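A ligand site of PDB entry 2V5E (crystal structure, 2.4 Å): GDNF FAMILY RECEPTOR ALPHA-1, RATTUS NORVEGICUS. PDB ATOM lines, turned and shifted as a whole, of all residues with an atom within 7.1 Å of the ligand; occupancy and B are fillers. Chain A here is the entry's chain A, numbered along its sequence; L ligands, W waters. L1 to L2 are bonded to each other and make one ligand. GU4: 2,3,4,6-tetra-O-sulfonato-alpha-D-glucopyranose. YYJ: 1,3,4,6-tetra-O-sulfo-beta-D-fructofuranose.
Water W5 lies within hydrogen-bond range of an oxygen (O22) of GU4 L1 and the backbone NH (N) of Tyr 105. Water W2 lies within hydrogen-bond range of an oxygen (O2S4) of YYJ L2 and the side-chain amino group of Lys 53. Water W1 bridges the side-chain amide oxygen (OD1) of Asn 104 (2.6 Å) and an oxygen (O24) of GU4 L1 (3.1 Å). Water W4 lies within hydrogen-bond range of the backbone carbonyl oxygen of Arg 41, the guanidinium group of Arg 48 and an oxygen (O29) of GU4 L1.
O27 of GU4 L1 is in salt-bridge range of NZ of Lys 45 (2.7 Å). The side-chain amide nitrogen of Gln 49 is in hydrogen-bond range of an oxygen (O3S3) of YYJ L2. The guanidinium group of Arg 48 lies within salt-bridge range of an oxygen (O1S3) of YYJ L2 (2.7 Å). The side-chain amide nitrogen of Asn 104 sits at hydrogen-bond distance from an oxygen (O26) of GU4 L1, 2.7 Å away. The side-chain amino group of Lys 53 is in salt-bridge range of an oxygen (O3S4) of YYJ L2, 3.0 Å away. NH1 of Arg 41 lies within salt-bridge range of O28 of GU4 L1. An oxygen (O23) of GU4 L1 lies within hydrogen-bond range of the backbone NH of Ile 106 (3.5 Å).
NH1 of Arg 48 lies within hydrogen-bond range of O of Gly 145 (2.9 Å). The backbone NH (N) of Ile 106 lies within hydrogen-bond range of the side-chain amide oxygen (OD1) of Asn 104 (3.2 Å). The side-chain amide oxygen (OD1) of Asn 104 sits at hydrogen-bond distance from the backbone NH (N) of Cys 107 (2.9 Å).
Merely in contact with the ligand: Tyr 105 (3.3 Å). Hydrophobic or aromatic side chains that line the ligand: Tyr 105 and Ile 106. Of the 18 residues printed, 8 come within 4 Å of the ligand. The nearest printed residue that does not touch the ligand is Asp 52 (4.5 Å).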
ATOM      1  N   ARG A  41      24.766  12.615   0.630  1.00  0.00           N
ATOM      2  CA  ARG A  41      25.990  13.126   1.253  1.00  0.00           C
ATOM      3  C   ARG A  41      26.408  14.483   0.673  1.00  0.00           C
ATOM      4  O   ARG A  41      26.703  15.423   1.413  1.00  0.00           O
ATOM      5  CB  ARG A  41      27.141  12.107   1.158  1.00  0.00           C
ATOM      6  CG  ARG A  41      28.496  12.646   1.654  1.00  0.00           C
ATOM      7  CD  ARG A  41      29.638  11.628   1.607  1.00  0.00           C
ATOM      8  NE  ARG A  41      30.323  11.592   0.316  1.00  0.00           N
ATOM      9  CZ  ARG A  41      30.788  12.668  -0.312  1.00  0.00           C
ATOM     10  NH1 ARG A  41      30.621  13.867   0.207  1.00  0.00           N
ATOM     11  NH2 ARG A  41      31.393  12.540  -1.479  1.00  0.00           N
ATOM     12  N   LYS A  42      26.460  14.584  -0.648  1.00  0.00           N
ATOM     13  CA  LYS A  42      26.886  15.819  -1.350  1.00  0.00           C
ATOM     14  C   LYS A  42      25.849  16.934  -1.186  1.00  0.00           C
ATOM     15  O   LYS A  42      26.195  18.109  -1.118  1.00  0.00           O
ATOM     16  CB  LYS A  42      27.093  15.571  -2.841  1.00  0.00           C
ATOM     17  CG  LYS A  42      28.296  14.709  -3.202  1.00  0.00           C
ATOM     18  CD  LYS A  42      28.557  14.770  -4.723  1.00  0.00           C
ATOM     19  CE  LYS A  42      29.861  14.045  -5.105  1.00  0.00           C
ATOM     20  NZ  LYS A  42      30.077  14.002  -6.592  1.00  0.00           N
ATOM     21  N   HIS A  44      23.742  17.138   1.502  1.00  0.00           N
ATOM     22  CA  HIS A  44      23.990  17.506   2.904  1.00  0.00           C
ATOM     23  C   HIS A  44      25.180  18.453   3.068  1.00  0.00           C
ATOM     24  O   HIS A  44      25.051  19.516   3.693  1.00  0.00           O
ATOM     25  CB  HIS A  44      24.118  16.248   3.775  1.00  0.00           C
ATOM     26  CG  HIS A  44      22.801  15.677   4.213  1.00  0.00           C
ATOM     27  ND1 HIS A  44      22.706  14.594   5.070  1.00  0.00           N
ATOM     28  CD2 HIS A  44      21.523  16.061   3.943  1.00  0.00           C
ATOM     29  CE1 HIS A  44      21.423  14.335   5.304  1.00  0.00           C
ATOM     30  NE2 HIS A  44      20.692  15.201   4.635  1.00  0.00           N
ATOM     31  N   LYS A  45      26.300  18.097   2.453  1.00  0.00           N
ATOM     32  CA  LYS A  45      27.501  18.940   2.495  1.00  0.00           C
ATOM     33  C   LYS A  45      27.229  20.370   2.050  1.00  0.00           C
ATOM     34  O   LYS A  45      27.545  21.324   2.768  1.00  0.00           O
ATOM     35  CB  LYS A  45      28.610  18.322   1.636  1.00  0.00           C
ATOM     36  CG  LYS A  45      29.991  18.893   1.855  1.00  0.00           C
ATOM     37  CD  LYS A  45      30.984  18.166   0.973  1.00  0.00           C
ATOM     38  CE  LYS A  45      32.338  18.852   0.942  1.00  0.00           C
ATOM     39  NZ  LYS A  45      33.112  18.557   2.165  1.00  0.00           N
ATOM     40  N   ALA A  46      26.619  20.520   0.881  1.00  0.00           N
ATOM     41  CA  ALA A  46      26.346  21.830   0.324  1.00  0.00           C
ATOM     42  C   ALA A  46      25.355  22.617   1.190  1.00  0.00           C
ATOM     43  O   ALA A  46      25.467  23.843   1.317  1.00  0.00           O
ATOM     44  CB  ALA A  46      25.863  21.705  -1.103  1.00  0.00           C
ATOM     45  N   LEU A  47      24.400  21.906   1.815  1.00  0.00           N
ATOM     46  CA  LEU A  47      23.466  22.547   2.757  1.00  0.00           C
ATOM     47  C   LEU A  47      24.181  23.142   3.972  1.00  0.00           C
ATOM     48  O   LEU A  47      23.898  24.276   4.351  1.00  0.00           O
ATOM     49  CB  LEU A  47      22.353  21.581   3.191  1.00  0.00           C
ATOM     50  CG  LEU A  47      21.195  21.393   2.187  1.00  0.00           C
ATOM     51  CD1 LEU A  47      20.429  20.122   2.508  1.00  0.00           C
ATOM     52  CD2 LEU A  47      20.260  22.579   2.194  1.00  0.00           C
ATOM     53  N   ARG A  48      25.086  22.364   4.558  1.00  0.00           N
ATOM     54  CA  ARG A  48      25.908  22.819   5.689  1.00  0.00           C
ATOM     55  C   ARG A  48      26.715  24.053   5.297  1.00  0.00           C
ATOM     56  O   ARG A  48      26.688  25.067   5.993  1.00  0.00           O
ATOM     57  CB  ARG A  48      26.839  21.706   6.190  1.00  0.00           C
ATOM     58  CG  ARG A  48      26.141  20.567   6.932  1.00  0.00           C
ATOM     59  CD  ARG A  48      27.126  19.665   7.702  1.00  0.00           C
ATOM     60  NE  ARG A  48      28.250  19.232   6.874  1.00  0.00           N
ATOM     61  CZ  ARG A  48      28.266  18.133   6.126  1.00  0.00           C
ATOM     62  NH1 ARG A  48      27.220  17.321   6.077  1.00  0.00           N
ATOM     63  NH2 ARG A  48      29.364  17.838   5.420  1.00  0.00           N
ATOM     64  N   GLN A  49      27.408  23.970   4.148  1.00  0.00           N
ATOM     65  CA  GLN A  49      28.158  25.120   3.630  1.00  0.00           C
ATOM     66  C   GLN A  49      27.281  26.337   3.386  1.00  0.00           C
ATOM     67  O   GLN A  49      27.705  27.452   3.691  1.00  0.00           O
ATOM     68  CB  GLN A  49      28.960  24.749   2.365  1.00  0.00           C
ATOM     69  CG  GLN A  49      29.913  23.547   2.577  1.00  0.00           C
ATOM     70  CD  GLN A  49      30.968  23.386   1.487  1.00  0.00           C
ATOM     71  OE1 GLN A  49      30.778  23.779   0.337  1.00  0.00           O
ATOM     72  NE2 GLN A  49      32.103  22.806   1.854  1.00  0.00           N
ATOM     73  N   ASP A  52      26.578  27.756   6.930  1.00  0.00           N
ATOM     74  CA  ASP A  52      27.828  28.172   7.571  1.00  0.00           C
ATOM     75  C   ASP A  52      28.467  29.365   6.864  1.00  0.00           C
ATOM     76  O   ASP A  52      29.078  30.202   7.510  1.00  0.00           O
ATOM     77  CB  ASP A  52      28.822  26.994   7.620  1.00  0.00           C
ATOM     78  CG  ASP A  52      30.021  27.259   8.535  1.00  0.00           C
ATOM     79  OD1 ASP A  52      29.840  27.725   9.693  1.00  0.00           O
ATOM     80  OD2 ASP A  52      31.149  26.967   8.083  1.00  0.00           O
ATOM     81  N   LYS A  53      28.295  29.457   5.547  1.00  0.00           N
ATOM     82  CA  LYS A  53      29.020  30.467   4.773  1.00  0.00           C
ATOM     83  C   LYS A  53      28.199  31.686   4.418  1.00  0.00           C
ATOM     84  O   LYS A  53      28.765  32.740   4.159  1.00  0.00           O
ATOM     85  CB  LYS A  53      29.680  29.855   3.539  1.00  0.00           C
ATOM     86  CG  LYS A  53      30.920  29.005   3.839  1.00  0.00           C
ATOM     87  CD  LYS A  53      31.820  29.706   4.886  1.00  0.00           C
ATOM     88  CE  LYS A  53      33.294  29.319   4.784  1.00  0.00           C
ATOM     89  NZ  LYS A  53      33.502  27.874   4.850  1.00  0.00           N
ATOM     90  N   THR A 103      27.741   9.751  16.773  1.00  0.00           N
ATOM     91  CA  THR A 103      29.041   9.226  16.302  1.00  0.00           C
ATOM     92  C   THR A 103      29.746  10.211  15.351  1.00  0.00           C
ATOM     93  O   THR A 103      30.877   9.983  14.928  1.00  0.00           O
ATOM     94  CB  THR A 103      28.902   7.872  15.558  1.00  0.00           C
ATOM     95  OG1 THR A 103      28.238   8.078  14.301  1.00  0.00           O
ATOM     96  CG2 THR A 103      28.112   6.832  16.412  1.00  0.00           C
ATOM     97  N   ASN A 104      29.069  11.308  15.021  1.00  0.00           N
ATOM     98  CA  ASN A 104      29.606  12.277  14.092  1.00  0.00           C
ATOM     99  C   ASN A 104      29.863  13.582  14.810  1.00  0.00           C
ATOM    100  O   ASN A 104      28.979  14.101  15.509  1.00  0.00           O
ATOM    101  CB  ASN A 104      28.647  12.505  12.912  1.00  0.00           C
ATOM    102  CG  ASN A 104      29.149  13.560  11.960  1.00  0.00           C
ATOM    103  OD1 ASN A 104      28.703  14.718  11.992  1.00  0.00           O
ATOM    104  ND2 ASN A 104      30.123  13.184  11.138  1.00  0.00           N
ATOM    105  N   TYR A 105      31.074  14.121  14.648  1.00  0.00           N
ATOM    106  CA  TYR A 105      31.462  15.300  15.419  1.00  0.00           C
ATOM    107  C   TYR A 105      30.488  16.466  15.196  1.00  0.00           C
ATOM    108  O   TYR A 105      30.021  17.073  16.156  1.00  0.00           O
ATOM    109  CB  TYR A 105      32.913  15.728  15.167  1.00  0.00           C
ATOM    110  CG  TYR A 105      33.137  17.163  15.564  1.00  0.00           C
ATOM    111  CD1 TYR A 105      33.147  17.545  16.917  1.00  0.00           C
ATOM    112  CD2 TYR A 105      33.319  18.159  14.598  1.00  0.00           C
ATOM    113  CE1 TYR A 105      33.318  18.862  17.298  1.00  0.00           C
ATOM    114  CE2 TYR A 105      33.485  19.484  14.974  1.00  0.00           C
ATOM    115  CZ  TYR A 105      33.486  19.831  16.326  1.00  0.00           C
ATOM    116  OH  TYR A 105      33.684  21.142  16.712  1.00  0.00           O
ATOM    117  N   ILE A 106      30.196  16.779  13.931  1.00  0.00           N
ATOM    118  CA  ILE A 106      29.343  17.933  13.633  1.00  0.00           C
ATOM    119  C   ILE A 106      27.905  17.694  14.143  1.00  0.00           C
ATOM    120  O   ILE A 106      27.316  18.563  14.799  1.00  0.00           O
ATOM    121  CB  ILE A 106      29.294  18.217  12.111  1.00  0.00           C
ATOM    122  CG1 ILE A 106      30.624  18.793  11.609  1.00  0.00           C
ATOM    123  CG2 ILE A 106      28.100  19.146  11.781  1.00  0.00           C
ATOM    124  CD1 ILE A 106      30.672  19.001  10.104  1.00  0.00           C
ATOM    125  N   CYS A 107      27.368  16.515  13.856  1.00  0.00           N
ATOM    126  CA  CYS A 107      26.013  16.207  14.307  1.00  0.00           C
ATOM    127  C   CYS A 107      25.900  16.249  15.832  1.00  0.00           C
ATOM    128  O   CYS A 107      25.034  16.947  16.371  1.00  0.00           O
ATOM    129  CB  CYS A 107      25.500  14.871  13.752  1.00  0.00           C
ATOM    130  SG  CYS A 107      23.687  14.791  13.796  1.00  0.00           S
ATOM    131  N   ARG A 110      26.085  20.008  16.957  1.00  0.00           N
ATOM    132  CA  ARG A 110      24.880  20.747  16.564  1.00  0.00           C
ATOM    133  C   ARG A 110      23.636  20.267  17.341  1.00  0.00           C
ATOM    134  O   ARG A 110      22.822  21.068  17.798  1.00  0.00           O
ATOM    135  CB  ARG A 110      24.642  20.629  15.050  1.00  0.00           C
ATOM    136  CG  ARG A 110      25.809  21.100  14.157  1.00  0.00           C
ATOM    137  CD  ARG A 110      25.966  22.587  14.116  1.00  0.00           C
ATOM    138  NE  ARG A 110      27.108  23.025  13.318  1.00  0.00           N
ATOM    139  CZ  ARG A 110      27.101  23.258  12.002  1.00  0.00           C
ATOM    140  NH1 ARG A 110      26.009  23.082  11.271  1.00  0.00           N
ATOM    141  NH2 ARG A 110      28.198  23.676  11.399  1.00  0.00           N
ATOM    142  N   GLY A 145      21.587  19.336   7.005  1.00  0.00           N
ATOM    143  CA  GLY A 145      22.758  18.718   6.426  1.00  0.00           C
ATOM    144  C   GLY A 145      23.424  17.688   7.341  1.00  0.00           C
ATOM    145  O   GLY A 145      24.487  17.170   7.008  1.00  0.00           O
ATOM    146  N   THR A 146      22.817  17.415   8.495  1.00  0.00           N
ATOM    147  CA  THR A 146      23.275  16.291   9.338  1.00  0.00           C
ATOM    148  C   THR A 146      22.244  15.183   9.191  1.00  0.00           C
ATOM    149  O   THR A 146      21.200  15.418   8.601  1.00  0.00           O
ATOM    150  CB  THR A 146      23.411  16.681  10.821  1.00  0.00           C
ATOM    151  OG1 THR A 146      22.110  16.854  11.389  1.00  0.00           O
ATOM    152  CG2 THR A 146      24.210  17.977  10.981  1.00  0.00           C
HETATM  153  C1  GU4 L   1      35.157  17.708   6.292  1.00  0.00           C
HETATM  154  O5  GU4 L   1      34.848  17.367   7.641  1.00  0.00           O
HETATM  155  C5  GU4 L   1      33.408  17.180   7.849  1.00  0.00           C
HETATM  156  C6  GU4 L   1      33.191  16.916   9.317  1.00  0.00           C
HETATM  157  O6  GU4 L   1      33.912  15.770   9.754  1.00  0.00           O
HETATM  158  S6  GU4 L   1      34.082  15.527  11.176  1.00  0.00           S
HETATM  159  O22 GU4 L   1      34.741  14.178  11.363  1.00  0.00           O
HETATM  160  O23 GU4 L   1      32.709  15.530  11.849  1.00  0.00           O
HETATM  161  O21 GU4 L   1      34.937  16.642  11.803  1.00  0.00           O
HETATM  162  C4  GU4 L   1      32.860  16.034   6.980  1.00  0.00           C
HETATM  163  O4  GU4 L   1      31.421  15.999   7.046  1.00  0.00           O
HETATM  164  S4  GU4 L   1      30.711  14.885   7.637  1.00  0.00           S
HETATM  165  O25 GU4 L   1      31.177  13.562   7.050  1.00  0.00           O
HETATM  166  O26 GU4 L   1      30.949  14.862   9.127  1.00  0.00           O
HETATM  167  O24 GU4 L   1      29.226  15.090   7.390  1.00  0.00           O
HETATM  168  C3  GU4 L   1      33.226  16.277   5.517  1.00  0.00           C
HETATM  169  O3  GU4 L   1      32.760  15.139   4.741  1.00  0.00           O
HETATM  170  S3  GU4 L   1      32.001  15.272   3.472  1.00  0.00           S
HETATM  171  O28 GU4 L   1      31.617  13.880   3.031  1.00  0.00           O
HETATM  172  O29 GU4 L   1      30.755  16.143   3.668  1.00  0.00           O
HETATM  173  O27 GU4 L   1      32.866  15.923   2.389  1.00  0.00           O
HETATM  174  C2  GU4 L   1      34.739  16.540   5.367  1.00  0.00           C
HETATM  175  O2  GU4 L   1      35.071  16.899   4.005  1.00  0.00           O
HETATM  176  S2  GU4 L   1      36.316  16.422   3.355  1.00  0.00           S
HETATM  177  O11 GU4 L   1      36.317  14.894   3.365  1.00  0.00           O
HETATM  178  O12 GU4 L   1      36.380  16.944   1.925  1.00  0.00           O
HETATM  179  O10 GU4 L   1      37.515  16.934   4.123  1.00  0.00           O
HETATM  180  C1  YYJ L   2      36.213  20.361   4.935  1.00  0.00           C
HETATM  181  C2  YYJ L   2      35.127  20.203   6.039  1.00  0.00           C
HETATM  182  C3  YYJ L   2      34.101  21.348   5.914  1.00  0.00           C
HETATM  183  C4  YYJ L   2      34.601  22.401   6.895  1.00  0.00           C
HETATM  184  C5  YYJ L   2      35.221  21.570   8.000  1.00  0.00           C
HETATM  185  C6  YYJ L   2      34.139  21.393   9.093  1.00  0.00           C
HETATM  186  O1  YYJ L   2      35.672  20.175   3.597  1.00  0.00           O
HETATM  187 O1S1 YYJ L   2      37.693  20.270   2.197  1.00  0.00           O
HETATM  188 O1S3 YYJ L   2      30.358  20.824   6.154  1.00  0.00           O
HETATM  189 O1S4 YYJ L   2      35.299  25.207   7.737  1.00  0.00           O
HETATM  190 O1S6 YYJ L   2      34.205  22.085  12.031  1.00  0.00           O
HETATM  191  O2  YYJ L   2      34.439  18.933   5.946  1.00  0.00           O
HETATM  192 O2S1 YYJ L   2      35.440  20.463   1.183  1.00  0.00           O
HETATM  193 O2S3 YYJ L   2      31.801  19.164   4.998  1.00  0.00           O
HETATM  194 O2S4 YYJ L   2      36.842  25.183   5.793  1.00  0.00           O
HETATM  195 O2S6 YYJ L   2      35.636  20.013  12.194  1.00  0.00           O
HETATM  196  O3  YYJ L   2      32.783  20.914   6.330  1.00  0.00           O
HETATM  197 O3S1 YYJ L   2      36.347  22.323   2.584  1.00  0.00           O
HETATM  198 O3S3 YYJ L   2      31.768  21.482   4.174  1.00  0.00           O
HETATM  199 O3S4 YYJ L   2      34.382  25.123   5.473  1.00  0.00           O
HETATM  200 O3S6 YYJ L   2      36.417  22.008  10.959  1.00  0.00           O
HETATM  201  O4  YYJ L   2      35.620  23.214   6.335  1.00  0.00           O
HETATM  202  O5  YYJ L   2      35.680  20.309   7.370  1.00  0.00           O
HETATM  203  O6  YYJ L   2      34.618  20.595  10.161  1.00  0.00           O
HETATM  204  S1  YYJ L   2      36.281  20.816   2.409  1.00  0.00           S
HETATM  205  S3  YYJ L   2      31.685  20.609   5.421  1.00  0.00           S
HETATM  206  S4  YYJ L   2      35.529  24.655   6.347  1.00  0.00           S
HETATM  207  S6  YYJ L   2      35.199  21.174  11.325  1.00  0.00           S
HETATM  208  O   HOH W   1      27.484  15.692   9.856  1.00  0.00           O
HETATM  209  O   HOH W   2      36.454  27.690   4.505  1.00  0.00           O
HETATM  210  O   HOH W   3      38.457  23.689   4.330  1.00  0.00           O
HETATM  211  O   HOH W   4      27.547  15.001   3.941  1.00  0.00           O
HETATM  212  O   HOH W   5      33.268  12.553  13.099  1.00  0.00           O
HETATM  213  O   HOH W   6      36.339  15.664  13.895  1.00  0.00           O
HETATM  214  O   HOH W   7      39.089  21.079   4.355  1.00  0.00           O
